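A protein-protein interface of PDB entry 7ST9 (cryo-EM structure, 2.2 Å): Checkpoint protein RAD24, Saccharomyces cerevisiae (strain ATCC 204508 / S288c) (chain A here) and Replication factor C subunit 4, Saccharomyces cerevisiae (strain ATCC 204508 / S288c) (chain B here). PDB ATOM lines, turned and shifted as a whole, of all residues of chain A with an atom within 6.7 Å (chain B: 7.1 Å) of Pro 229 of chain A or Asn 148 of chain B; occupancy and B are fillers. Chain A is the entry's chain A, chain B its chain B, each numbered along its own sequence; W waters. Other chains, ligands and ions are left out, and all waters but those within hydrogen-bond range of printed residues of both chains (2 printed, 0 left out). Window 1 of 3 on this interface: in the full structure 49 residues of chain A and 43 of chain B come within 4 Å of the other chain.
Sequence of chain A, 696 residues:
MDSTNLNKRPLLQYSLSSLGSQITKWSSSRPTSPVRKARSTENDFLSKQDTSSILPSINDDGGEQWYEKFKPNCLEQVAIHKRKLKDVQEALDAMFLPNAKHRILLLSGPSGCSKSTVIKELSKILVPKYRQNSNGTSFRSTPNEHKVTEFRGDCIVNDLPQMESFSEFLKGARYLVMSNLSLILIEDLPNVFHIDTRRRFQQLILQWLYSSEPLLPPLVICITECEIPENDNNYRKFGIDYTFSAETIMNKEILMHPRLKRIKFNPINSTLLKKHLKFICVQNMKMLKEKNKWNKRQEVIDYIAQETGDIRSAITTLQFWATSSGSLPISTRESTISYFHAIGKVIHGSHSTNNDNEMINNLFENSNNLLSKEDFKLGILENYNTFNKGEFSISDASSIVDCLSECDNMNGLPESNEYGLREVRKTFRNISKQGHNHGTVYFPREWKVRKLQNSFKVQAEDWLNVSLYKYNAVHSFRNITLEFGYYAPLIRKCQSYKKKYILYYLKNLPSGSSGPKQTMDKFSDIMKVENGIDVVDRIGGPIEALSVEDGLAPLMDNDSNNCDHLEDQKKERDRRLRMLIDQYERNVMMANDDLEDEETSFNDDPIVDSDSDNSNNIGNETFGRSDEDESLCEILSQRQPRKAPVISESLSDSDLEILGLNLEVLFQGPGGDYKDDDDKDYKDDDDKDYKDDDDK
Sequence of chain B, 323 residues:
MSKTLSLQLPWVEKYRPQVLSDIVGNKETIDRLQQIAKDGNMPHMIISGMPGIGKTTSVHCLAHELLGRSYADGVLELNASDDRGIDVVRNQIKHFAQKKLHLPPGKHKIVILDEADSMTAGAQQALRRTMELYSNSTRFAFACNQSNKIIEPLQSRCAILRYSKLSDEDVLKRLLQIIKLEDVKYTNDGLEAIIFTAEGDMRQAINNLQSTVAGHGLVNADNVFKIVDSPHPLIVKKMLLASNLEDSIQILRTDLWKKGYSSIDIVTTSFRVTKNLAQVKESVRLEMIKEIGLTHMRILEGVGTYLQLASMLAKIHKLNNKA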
ATOM      1  N   GLU A 227     -18.230  -8.261 -23.995  1.00  0.00           N
ATOM      2  CA  GLU A 227     -18.877  -7.620 -25.130  1.00  0.00           C
ATOM      3  C   GLU A 227     -17.825  -7.174 -26.136  1.00  0.00           C
ATOM      4  O   GLU A 227     -16.728  -6.753 -25.760  1.00  0.00           O
ATOM      5  CB  GLU A 227     -19.713  -6.419 -24.680  1.00  0.00           C
ATOM      6  CG  GLU A 227     -20.251  -6.507 -23.257  1.00  0.00           C
ATOM      7  CD  GLU A 227     -20.920  -7.838 -22.958  1.00  0.00           C
ATOM      8  OE1 GLU A 227     -21.546  -8.410 -23.873  1.00  0.00           O
ATOM      9  OE2 GLU A 227     -20.817  -8.309 -21.805  1.00  0.00           O
ATOM     10  N   ILE A 228     -18.163  -7.284 -27.417  1.00  0.00           N
ATOM     11  CA  ILE A 228     -17.279  -6.863 -28.500  1.00  0.00           C
ATOM     12  C   ILE A 228     -17.582  -5.396 -28.798  1.00  0.00           C
ATOM     13  O   ILE A 228     -18.684  -5.095 -29.287  1.00  0.00           O
ATOM     14  CB  ILE A 228     -17.472  -7.730 -29.752  1.00  0.00           C
ATOM     15  CG1 ILE A 228     -17.243  -9.210 -29.424  1.00  0.00           C
ATOM     16  CG2 ILE A 228     -16.538  -7.276 -30.865  1.00  0.00           C
ATOM     17  CD1 ILE A 228     -15.883  -9.514 -28.827  1.00  0.00           C
ATOM     18  N   PRO A 229     -16.664  -4.468 -28.525  1.00  0.00           N
ATOM     19  CA  PRO A 229     -16.934  -3.064 -28.852  1.00  0.00           C
ATOM     20  C   PRO A 229     -17.141  -2.875 -30.347  1.00  0.00           C
ATOM     21  O   PRO A 229     -16.517  -3.542 -31.174  1.00  0.00           O
ATOM     22  CB  PRO A 229     -15.678  -2.333 -28.361  1.00  0.00           C
ATOM     23  CG  PRO A 229     -15.056  -3.253 -27.369  1.00  0.00           C
ATOM     24  CD  PRO A 229     -15.366  -4.632 -27.849  1.00  0.00           C
ATOM     25  N   GLU A 230     -18.038  -1.953 -30.686  1.00  0.00           N
ATOM     26  CA  GLU A 230     -18.320  -1.670 -32.086  1.00  0.00           C
ATOM     27  C   GLU A 230     -17.047  -1.217 -32.791  1.00  0.00           C
ATOM     28  O   GLU A 230     -16.341  -0.325 -32.312  1.00  0.00           O
ATOM     29  CB  GLU A 230     -19.405  -0.594 -32.193  1.00  0.00           C
ATOM     30  CG  GLU A 230     -20.015  -0.325 -33.589  1.00  0.00           C
ATOM     31  CD  GLU A 230     -20.098  -1.531 -34.520  1.00  0.00           C
ATOM     32  OE1 GLU A 230     -20.049  -2.685 -34.052  1.00  0.00           O
ATOM     33  OE2 GLU A 230     -20.214  -1.316 -35.746  1.00  0.00           O
ATOM     34  N   ASN A 231     -16.762  -1.831 -33.937  1.00  0.00           N
ATOM     35  CA  ASN A 231     -15.535  -1.577 -34.678  1.00  0.00           C
ATOM     36  C   ASN A 231     -15.878  -1.151 -36.097  1.00  0.00           C
ATOM     37  O   ASN A 231     -16.823  -1.669 -36.700  1.00  0.00           O
ATOM     38  CB  ASN A 231     -14.637  -2.821 -34.704  1.00  0.00           C
ATOM     39  CG  ASN A 231     -13.168  -2.481 -34.874  1.00  0.00           C
ATOM     40  OD1 ASN A 231     -12.778  -1.313 -34.837  1.00  0.00           O
ATOM     41  ND2 ASN A 231     -12.343  -3.504 -35.063  1.00  0.00           N
ATOM     42  N   ASP A 232     -15.102  -0.203 -36.624  1.00  0.00           N
ATOM     43  CA  ASP A 232     -15.379   0.324 -37.956  1.00  0.00           C
ATOM     44  C   ASP A 232     -15.076  -0.696 -39.046  1.00  0.00           C
ATOM     45  O   ASP A 232     -15.697  -0.659 -40.114  1.00  0.00           O
ATOM     46  CB  ASP A 232     -14.568   1.598 -38.190  1.00  0.00           C
ATOM     47  CG  ASP A 232     -14.886   2.684 -37.182  1.00  0.00           C
ATOM     48  OD1 ASP A 232     -16.058   2.788 -36.765  1.00  0.00           O
ATOM     49  OD2 ASP A 232     -13.960   3.435 -36.808  1.00  0.00           O
ATOM     50  N   ASN A 234     -15.551  -3.960 -38.943  1.00  0.00           N
ATOM     51  CA  ASN A 234     -16.419  -5.135 -38.935  1.00  0.00           C
ATOM     52  C   ASN A 234     -17.720  -4.875 -39.691  1.00  0.00           C
ATOM     53  O   ASN A 234     -18.003  -5.537 -40.696  1.00  0.00           O
ATOM     54  CB  ASN A 234     -16.714  -5.557 -37.491  1.00  0.00           C
ATOM     55  CG  ASN A 234     -17.774  -6.636 -37.405  1.00  0.00           C
ATOM     56  OD1 ASN A 234     -17.766  -7.593 -38.179  1.00  0.00           O
ATOM     57  ND2 ASN A 234     -18.696  -6.487 -36.462  1.00  0.00           N
ATOM     58  N   ASP A 241     -20.366 -11.228 -33.234  1.00  0.00           N
ATOM     59  CA  ASP A 241     -19.727  -9.923 -33.371  1.00  0.00           C
ATOM     60  C   ASP A 241     -20.238  -8.914 -32.350  1.00  0.00           C
ATOM     61  O   ASP A 241     -19.608  -7.867 -32.171  1.00  0.00           O
ATOM     62  CB  ASP A 241     -19.930  -9.371 -34.782  1.00  0.00           C
ATOM     63  CG  ASP A 241     -19.623 -10.392 -35.858  1.00  0.00           C
ATOM     64  OD1 ASP A 241     -18.548 -11.025 -35.791  1.00  0.00           O
ATOM     65  OD2 ASP A 241     -20.457 -10.562 -36.769  1.00  0.00           O
ATOM     66  N   TYR A 242     -21.358  -9.196 -31.687  1.00  0.00           N
ATOM     67  CA  TYR A 242     -21.857  -8.321 -30.633  1.00  0.00           C
ATOM     68  C   TYR A 242     -21.385  -8.759 -29.253  1.00  0.00           C
ATOM     69  O   TYR A 242     -20.972  -7.921 -28.445  1.00  0.00           O
ATOM     70  CB  TYR A 242     -23.388  -8.277 -30.658  1.00  0.00           C
ATOM     71  CG  TYR A 242     -23.964  -7.332 -31.687  1.00  0.00           C
ATOM     72  CD1 TYR A 242     -23.743  -5.964 -31.604  1.00  0.00           C
ATOM     73  CD2 TYR A 242     -24.737  -7.807 -32.737  1.00  0.00           C
ATOM     74  CE1 TYR A 242     -24.270  -5.096 -32.541  1.00  0.00           C
ATOM     75  CE2 TYR A 242     -25.270  -6.947 -33.678  1.00  0.00           C
ATOM     76  CZ  TYR A 242     -25.033  -5.593 -33.576  1.00  0.00           C
ATOM     77  OH  TYR A 242     -25.561  -4.734 -34.511  1.00  0.00           O
ATOM     78  N   GLU A 334     -13.010  -0.869 -16.761  1.00  0.00           N
ATOM     79  CA  GLU A 334     -14.453  -0.680 -16.803  1.00  0.00           C
ATOM     80  C   GLU A 334     -15.157  -2.019 -16.985  1.00  0.00           C
ATOM     81  O   GLU A 334     -14.660  -2.912 -17.679  1.00  0.00           O
ATOM     82  CB  GLU A 334     -14.838   0.279 -17.931  1.00  0.00           C
ATOM     83  CG  GLU A 334     -13.953   1.516 -18.037  1.00  0.00           C
ATOM     84  CD  GLU A 334     -12.867   1.380 -19.086  1.00  0.00           C
ATOM     85  OE1 GLU A 334     -11.917   0.602 -18.862  1.00  0.00           O
ATOM     86  OE2 GLU A 334     -12.957   2.060 -20.130  1.00  0.00           O
ATOM     87  N   THR A 336     -18.809  -3.761 -18.099  1.00  0.00           N
ATOM     88  CA  THR A 336     -20.101  -3.567 -18.741  1.00  0.00           C
ATOM     89  C   THR A 336     -21.220  -4.123 -17.867  1.00  0.00           C
ATOM     90  O   THR A 336     -21.038  -5.095 -17.129  1.00  0.00           O
ATOM     91  CB  THR A 336     -20.134  -4.249 -20.109  1.00  0.00           C
ATOM     92  OG1 THR A 336     -19.837  -5.643 -19.957  1.00  0.00           O
ATOM     93  CG2 THR A 336     -19.125  -3.611 -21.054  1.00  0.00           C
ATOM     94  N   GLU A 365     -22.646   6.216 -23.452  1.00  0.00           N
ATOM     95  CA  GLU A 365     -21.229   6.240 -23.797  1.00  0.00           C
ATOM     96  C   GLU A 365     -20.592   4.866 -23.638  1.00  0.00           C
ATOM     97  O   GLU A 365     -19.808   4.438 -24.494  1.00  0.00           O
ATOM     98  CB  GLU A 365     -20.501   7.269 -22.931  1.00  0.00           C
ATOM     99  CG  GLU A 365     -19.399   8.020 -23.660  1.00  0.00           C
ATOM    100  CD  GLU A 365     -18.681   9.011 -22.765  1.00  0.00           C
ATOM    101  OE1 GLU A 365     -18.965   9.030 -21.549  1.00  0.00           O
ATOM    102  OE2 GLU A 365     -17.832   9.771 -23.278  1.00  0.00           O
ATOM    103  N   ASN A 366     -20.914   4.156 -22.557  1.00  0.00           N
ATOM    104  CA  ASN A 366     -20.247   2.902 -22.232  1.00  0.00           C
ATOM    105  C   ASN A 366     -21.060   1.663 -22.587  1.00  0.00           C
ATOM    106  O   ASN A 366     -20.534   0.551 -22.475  1.00  0.00           O
ATOM    107  CB  ASN A 366     -19.905   2.865 -20.737  1.00  0.00           C
ATOM    108  CG  ASN A 366     -18.933   3.957 -20.337  1.00  0.00           C
ATOM    109  OD1 ASN A 366     -17.844   4.069 -20.900  1.00  0.00           O
ATOM    110  ND2 ASN A 366     -19.322   4.769 -19.362  1.00  0.00           N
ATOM    111  N   SER A 367     -22.314   1.817 -23.010  1.00  0.00           N
ATOM    112  CA  SER A 367     -23.166   0.677 -23.337  1.00  0.00           C
ATOM    113  C   SER A 367     -23.918   0.932 -24.636  1.00  0.00           C
ATOM    114  O   SER A 367     -25.096   0.587 -24.772  1.00  0.00           O
ATOM    115  CB  SER A 367     -24.146   0.378 -22.203  1.00  0.00           C
ATOM    116  OG  SER A 367     -23.524   0.535 -20.939  1.00  0.00           O
ATOM    117  N   ASN A 368     -23.240   1.538 -25.613  1.00  0.00           N
ATOM    118  CA  ASN A 368     -23.902   1.869 -26.871  1.00  0.00           C
ATOM    119  C   ASN A 368     -24.368   0.617 -27.601  1.00  0.00           C
ATOM    120  O   ASN A 368     -25.463   0.597 -28.174  1.00  0.00           O
ATOM    121  CB  ASN A 368     -22.964   2.685 -27.758  1.00  0.00           C
ATOM    122  CG  ASN A 368     -23.691   3.366 -28.900  1.00  0.00           C
ATOM    123  OD1 ASN A 368     -24.552   4.217 -28.681  1.00  0.00           O
ATOM    124  ND2 ASN A 368     -23.350   2.990 -30.127  1.00  0.00           N
ATOM    125  N   ASN A 369     -23.550  -0.437 -27.601  1.00  0.00           N
ATOM    126  CA  ASN A 369     -23.918  -1.656 -28.316  1.00  0.00           C
ATOM    127  C   ASN A 369     -25.237  -2.215 -27.797  1.00  0.00           C
ATOM    128  O   ASN A 369     -26.125  -2.575 -28.577  1.00  0.00           O
ATOM    129  CB  ASN A 369     -22.810  -2.699 -28.177  1.00  0.00           C
ATOM    130  CG  ASN A 369     -21.704  -2.515 -29.195  1.00  0.00           C
ATOM    131  OD1 ASN A 369     -21.958  -2.213 -30.360  1.00  0.00           O
ATOM    132  ND2 ASN A 369     -20.466  -2.709 -28.758  1.00  0.00           N
ATOM    133  N   SER B  48      -5.570   6.624 -22.522  1.00  0.00           N
ATOM    134  CA  SER B  48      -6.811   7.068 -23.138  1.00  0.00           C
ATOM    135  C   SER B  48      -6.976   8.573 -22.971  1.00  0.00           C
ATOM    136  O   SER B  48      -6.548   9.153 -21.969  1.00  0.00           O
ATOM    137  CB  SER B  48      -8.019   6.344 -22.529  1.00  0.00           C
ATOM    138  OG  SER B  48      -8.026   6.465 -21.117  1.00  0.00           O
ATOM    139  N   ASP B 117      -7.699   0.771 -30.315  1.00  0.00           N
ATOM    140  CA  ASP B 117      -9.144   0.573 -30.335  1.00  0.00           C
ATOM    141  C   ASP B 117      -9.613  -0.029 -31.654  1.00  0.00           C
ATOM    142  O   ASP B 117     -10.595  -0.781 -31.677  1.00  0.00           O
ATOM    143  CB  ASP B 117      -9.856   1.902 -30.075  1.00  0.00           C
ATOM    144  CG  ASP B 117      -9.264   3.049 -30.871  1.00  0.00           C
ATOM    145  OD1 ASP B 117      -9.466   3.085 -32.103  1.00  0.00           O
ATOM    146  OD2 ASP B 117      -8.596   3.912 -30.263  1.00  0.00           O
ATOM    147  N   MET B 119      -8.247  -2.306 -33.438  1.00  0.00           N
ATOM    148  CA  MET B 119      -7.867  -3.695 -33.655  1.00  0.00           C
ATOM    149  C   MET B 119      -9.102  -4.587 -33.720  1.00  0.00           C
ATOM    150  O   MET B 119     -10.092  -4.359 -33.020  1.00  0.00           O
ATOM    151  CB  MET B 119      -6.936  -4.167 -32.538  1.00  0.00           C
ATOM    152  CG  MET B 119      -5.552  -3.535 -32.580  1.00  0.00           C
ATOM    153  SD  MET B 119      -4.316  -4.494 -31.684  1.00  0.00           S
ATOM    154  CE  MET B 119      -4.047  -5.856 -32.816  1.00  0.00           C
ATOM    155  N   ALA B 121     -11.563  -7.932 -33.382  1.00  0.00           N
ATOM    156  CA  ALA B 121     -11.885  -8.757 -32.222  1.00  0.00           C
ATOM    157  C   ALA B 121     -11.003  -9.997 -32.160  1.00  0.00           C
ATOM    158  O   ALA B 121     -10.518 -10.371 -31.086  1.00  0.00           O
ATOM    159  CB  ALA B 121     -13.362  -9.151 -32.256  1.00  0.00           C
ATOM    160  N   GLN B 124      -7.523  -9.044 -30.959  1.00  0.00           N
ATOM    161  CA  GLN B 124      -7.540  -8.725 -29.536  1.00  0.00           C
ATOM    162  C   GLN B 124      -7.624  -9.991 -28.694  1.00  0.00           C
ATOM    163  O   GLN B 124      -6.923 -10.121 -27.683  1.00  0.00           O
ATOM    164  CB  GLN B 124      -8.707  -7.790 -29.221  1.00  0.00           C
ATOM    165  CG  GLN B 124      -8.483  -6.355 -29.672  1.00  0.00           C
ATOM    166  CD  GLN B 124      -9.366  -5.368 -28.938  1.00  0.00           C
ATOM    167  OE1 GLN B 124      -9.380  -5.325 -27.708  1.00  0.00           O
ATOM    168  NE2 GLN B 124     -10.108  -4.564 -29.689  1.00  0.00           N
ATOM    169  N   CYS B 144      -5.239   4.854 -27.136  1.00  0.00           N
ATOM    170  CA  CYS B 144      -6.565   4.899 -27.734  1.00  0.00           C
ATOM    171  C   CYS B 144      -7.270   6.165 -27.274  1.00  0.00           C
ATOM    172  O   CYS B 144      -6.797   6.880 -26.389  1.00  0.00           O
ATOM    173  CB  CYS B 144      -7.383   3.658 -27.365  1.00  0.00           C
ATOM    174  SG  CYS B 144      -7.488   3.348 -25.589  1.00  0.00           S
ATOM    175  N   ASN B 145      -8.408   6.439 -27.907  1.00  0.00           N
ATOM    176  CA  ASN B 145      -9.285   7.525 -27.491  1.00  0.00           C
ATOM    177  C   ASN B 145     -10.430   7.049 -26.611  1.00  0.00           C
ATOM    178  O   ASN B 145     -10.844   7.780 -25.705  1.00  0.00           O
ATOM    179  CB  ASN B 145      -9.853   8.241 -28.720  1.00  0.00           C
ATOM    180  CG  ASN B 145      -8.768   8.806 -29.617  1.00  0.00           C
ATOM    181  OD1 ASN B 145      -8.633   8.408 -30.773  1.00  0.00           O
ATOM    182  ND2 ASN B 145      -7.986   9.738 -29.085  1.00  0.00           N
ATOM    183  N   GLN B 146     -10.943   5.844 -26.851  1.00  0.00           N
ATOM    184  CA  GLN B 146     -12.005   5.248 -26.045  1.00  0.00           C
ATOM    185  C   GLN B 146     -11.443   3.999 -25.377  1.00  0.00           C
ATOM    186  O   GLN B 146     -11.222   2.981 -26.041  1.00  0.00           O
ATOM    187  CB  GLN B 146     -13.223   4.911 -26.906  1.00  0.00           C
ATOM    188  CG  GLN B 146     -13.706   6.060 -27.774  1.00  0.00           C
ATOM    189  CD  GLN B 146     -13.986   7.317 -26.976  1.00  0.00           C
ATOM    190  OE1 GLN B 146     -14.570   7.260 -25.892  1.00  0.00           O
ATOM    191  NE2 GLN B 146     -13.571   8.461 -27.506  1.00  0.00           N
ATOM    192  N   SER B 147     -11.215   4.079 -24.064  1.00  0.00           N
ATOM    193  CA  SER B 147     -10.634   2.949 -23.347  1.00  0.00           C
ATOM    194  C   SER B 147     -11.546   1.731 -23.378  1.00  0.00           C
ATOM    195  O   SER B 147     -11.062   0.594 -23.336  1.00  0.00           O
ATOM    196  CB  SER B 147     -10.335   3.348 -21.901  1.00  0.00           C
ATOM    197  OG  SER B 147      -9.464   2.414 -21.285  1.00  0.00           O
ATOM    198  N   ASN B 148     -12.862   1.941 -23.451  1.00  0.00           N
ATOM    199  CA  ASN B 148     -13.804   0.828 -23.448  1.00  0.00           C
ATOM    200  C   ASN B 148     -13.765   0.017 -24.736  1.00  0.00           C
ATOM    201  O   ASN B 148     -14.322  -1.086 -24.768  1.00  0.00           O
ATOM    202  CB  ASN B 148     -15.224   1.345 -23.213  1.00  0.00           C
ATOM    203  CG  ASN B 148     -15.749   2.158 -24.377  1.00  0.00           C
ATOM    204  OD1 ASN B 148     -15.093   3.091 -24.842  1.00  0.00           O
ATOM    205  ND2 ASN B 148     -16.938   1.812 -24.853  1.00  0.00           N
ATOM    206  N   LYS B 149     -13.125   0.522 -25.790  1.00  0.00           N
ATOM    207  CA  LYS B 149     -13.055  -0.208 -27.049  1.00  0.00           C
ATOM    208  C   LYS B 149     -12.009  -1.316 -27.028  1.00  0.00           C
ATOM    209  O   LYS B 149     -11.916  -2.075 -27.998  1.00  0.00           O
ATOM    210  CB  LYS B 149     -12.773   0.761 -28.201  1.00  0.00           C
ATOM    211  CG  LYS B 149     -13.987   1.008 -29.086  1.00  0.00           C
ATOM    212  CD  LYS B 149     -13.651   1.871 -30.298  1.00  0.00           C
ATOM    213  CE  LYS B 149     -13.238   1.053 -31.520  1.00  0.00           C
ATOM    214  NZ  LYS B 149     -14.075  -0.152 -31.764  1.00  0.00           N
ATOM    215  N   ILE B 150     -11.229  -1.426 -25.958  1.00  0.00           N
ATOM    216  CA  ILE B 150     -10.331  -2.555 -25.751  1.00  0.00           C
ATOM    217  C   ILE B 150     -11.061  -3.590 -24.904  1.00  0.00           C
ATOM    218  O   ILE B 150     -11.644  -3.256 -23.867  1.00  0.00           O
ATOM    219  CB  ILE B 150      -9.023  -2.103 -25.076  1.00  0.00           C
ATOM    220  CG1 ILE B 150      -8.335  -1.025 -25.921  1.00  0.00           C
ATOM    221  CG2 ILE B 150      -8.092  -3.292 -24.863  1.00  0.00           C
ATOM    222  CD1 ILE B 150      -7.188  -0.335 -25.221  1.00  0.00           C
ATOM    223  N   ILE B 151     -11.034  -4.850 -25.348  1.00  0.00           N
ATOM    224  CA  ILE B 151     -11.833  -5.878 -24.693  1.00  0.00           C
ATOM    225  C   ILE B 151     -11.415  -6.026 -23.231  1.00  0.00           C
ATOM    226  O   ILE B 151     -10.251  -5.825 -22.864  1.00  0.00           O
ATOM    227  CB  ILE B 151     -11.723  -7.221 -25.435  1.00  0.00           C
ATOM    228  CG1 ILE B 151     -10.274  -7.717 -25.463  1.00  0.00           C
ATOM    229  CG2 ILE B 151     -12.265  -7.084 -26.850  1.00  0.00           C
ATOM    230  CD1 ILE B 151     -10.125  -9.126 -25.999  1.00  0.00           C
ATOM    231  N   GLU B 152     -12.384  -6.387 -22.392  1.00  0.00           N
ATOM    232  CA  GLU B 152     -12.138  -6.463 -20.955  1.00  0.00           C
ATOM    233  C   GLU B 152     -11.003  -7.407 -20.580  1.00  0.00           C
ATOM    234  O   GLU B 152     -10.227  -7.060 -19.671  1.00  0.00           O
ATOM    235  CB  GLU B 152     -13.432  -6.870 -20.239  1.00  0.00           C
ATOM    236  CG  GLU B 152     -14.265  -5.686 -19.777  1.00  0.00           C
ATOM    237  CD  GLU B 152     -15.756  -5.965 -19.794  1.00  0.00           C
ATOM    238  OE1 GLU B 152     -16.148  -7.138 -19.963  1.00  0.00           O
ATOM    239  OE2 GLU B 152     -16.537  -5.005 -19.634  1.00  0.00           O
ATOM    240  N   GLN B 155      -7.934  -5.380 -20.869  1.00  0.00           N
ATOM    241  CA  GLN B 155      -7.923  -4.320 -19.867  1.00  0.00           C
ATOM    242  C   GLN B 155      -7.547  -4.853 -18.492  1.00  0.00           C
ATOM    243  O   GLN B 155      -6.927  -4.140 -17.697  1.00  0.00           O
ATOM    244  CB  GLN B 155      -9.294  -3.648 -19.804  1.00  0.00           C
ATOM    245  CG  GLN B 155      -9.593  -2.721 -20.962  1.00  0.00           C
ATOM    246  CD  GLN B 155     -10.936  -2.039 -20.814  1.00  0.00           C
ATOM    247  OE1 GLN B 155     -11.355  -1.708 -19.707  1.00  0.00           O
ATOM    248  NE2 GLN B 155     -11.620  -1.825 -21.930  1.00  0.00           N
ATOM    249  N   ARG B 162      -5.761   7.862 -17.878  1.00  0.00           N
ATOM    250  CA  ARG B 162      -6.666   8.724 -18.623  1.00  0.00           C
ATOM    251  C   ARG B 162      -6.108  10.141 -18.632  1.00  0.00           C
ATOM    252  O   ARG B 162      -5.838  10.714 -17.572  1.00  0.00           O
ATOM    253  CB  ARG B 162      -8.067   8.696 -18.010  1.00  0.00           C
ATOM    254  CG  ARG B 162      -8.606   7.291 -17.774  1.00  0.00           C
ATOM    255  CD  ARG B 162      -9.836   7.303 -16.883  1.00  0.00           C
ATOM    256  NE  ARG B 162     -10.346   5.960 -16.633  1.00  0.00           N
ATOM    257  CZ  ARG B 162     -10.940   5.198 -17.540  1.00  0.00           C
ATOM    258  NH1 ARG B 162     -11.123   5.616 -18.783  1.00  0.00           N
ATOM    259  NH2 ARG B 162     -11.363   3.985 -17.194  1.00  0.00           N
HETATM  260  O   HOH W   1     -14.963  -2.515 -20.494  1.00  0.00           O
HETATM  261  O   HOH W   2     -15.208  -6.357 -23.434  1.00  0.00           O
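Of chain B, only Asn 148 (3.5 Å) and Lys 149 (3.4 Å) come within 4 Å of Pro 229 of chain A.
Asn 148 of chain B touches just these residues of chain A: Pro 229, Glu 334 and Glu 365.
Of the printed residues of chain B, Thr 336 of chain A touches Glu 152.
Printed residues of chain B within 4 Å of Glu 365 of chain A: Asn 148 (3.9 Å).
Printed residues of chain A within 4 Å of Arg 162 of chain B: Glu 334.
Asn 368 of chain A touches none of the printed residues of chain B.
Cys 144 of chain B touches none of the printed residues of chain A.
The nearest residue of chain B that does not touch Pro 229 of chain A is Ile 151 of chain B (4.1 Å).
The nearest residue of chain A that does not touch Asn 148 of chain B is Asn 366 of chain A (4.4 Å).
The nearest printed residue of chain A that does not touch Ser 147 of chain B is Pro 229 of chain A (6.9 Å).
Water W2 bridges the backbone carbonyl oxygen (O) of Glu 227 of chain A (2.8 Å) and the backbone NH (N) of Glu 152 of chain B (3.0 Å).
Water W1 lies within hydrogen-bond range of O of Glu 334 of chain A and OE2 of Glu 152 of chain B.
Hydrophobic or aromatic side chains of chain B that line the printed part of chain A: Ala 121.
Along chain B the printed residues that touch a printed residue of chain A span positions 117 to 162.
Of the 16 printed residues of chain A, 7 touch a printed residue of chain B.
Printed residues of chain A that touch a printed residue of chain B: Ile 228, Pro 229, Glu 230, Asn 231, Glu 334, Thr 336 and Glu 365.
Hydrophobic or aromatic side chains of chain A that line the printed part of chain B: Ile 228 and Pro 229.
Among the printed residues, 14 pairs touch across the chains.
O of Ser 147 of chain B lies within hydrogen-bond range of NE2 of Gln 155 of chain B (2.9 Å).
The side-chain carboxylate of Glu 227 of chain A sits at hydrogen-bond distance from the side-chain hydroxyl of Thr 336 of chain A.
OD2 of Asp 117 of chain B is in hydrogen-bond range of N of Asn 145 of chain B (3.5 Å).
The backbone NH (N) of Ile 228 of chain A sits at hydrogen-bond distance from the backbone carbonyl oxygen (O) of Tyr 242 of chain A (3.1 Å).
The backbone carbonyl oxygen of Ile 150 of chain B sits at hydrogen-bond distance from the side-chain amide nitrogen of Gln 155 of chain B.
The backbone carbonyl oxygen (O) of Ile 228 of chain A sits at hydrogen-bond distance from the side-chain amide nitrogen (ND2) of Asn 369 of chain A (3.0 Å).
Ile 228 of chain A touches Ala 121 of chain B.
Pro 229 of chain A touches Asn 148 of chain B (CG to O, 3.5 Å).
Lys 149 of chain B touches Pro 229 of chain A (O to CG, 3.4 Å).
OD1 of Asn 231 of chain A touches O of Asp 117 of chain B, 3.9 Å away.
OD1 of Asn 231 of chain A touches NZ of Lys 149 of chain B (3.5 Å).
Ser 147 of chain B touches Glu 334 of chain A.
Glu 365 of chain A touches Asn 148 of chain B (O to ND2, 3.9 Å).
The side-chain amino group (NZ) of Lys 149 of chain B sits close to the backbone carbonyl oxygen (O) of Glu 230 of chain A.
The side-chain carboxylate (OE1) of Glu 334 of chain A lies within salt-bridge range of the guanidinium group (NH2) of Arg 162 of chain B.
The backbone carbonyl oxygen (O) of Glu 334 of chain A lies close to the side-chain carboxylate (OE2) of Glu 152 of chain B (3.4 Å).
The backbone NH of Thr 336 of chain A is in hydrogen-bond range of the side-chain carboxylate of Glu 152 of chain B, at 3.0 Å.
OE2 of Glu 334 of chain A sits at hydrogen-bond distance from N of Asn 148 of chain B (3.3 Å).
OE1 of Glu 334 of chain A sits close to OE1 of Gln 155 of chain B, at 2.5 Å.
ND2 of Asn 231 of chain A sits at hydrogen-bond distance from O of Met 119 of chain B.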
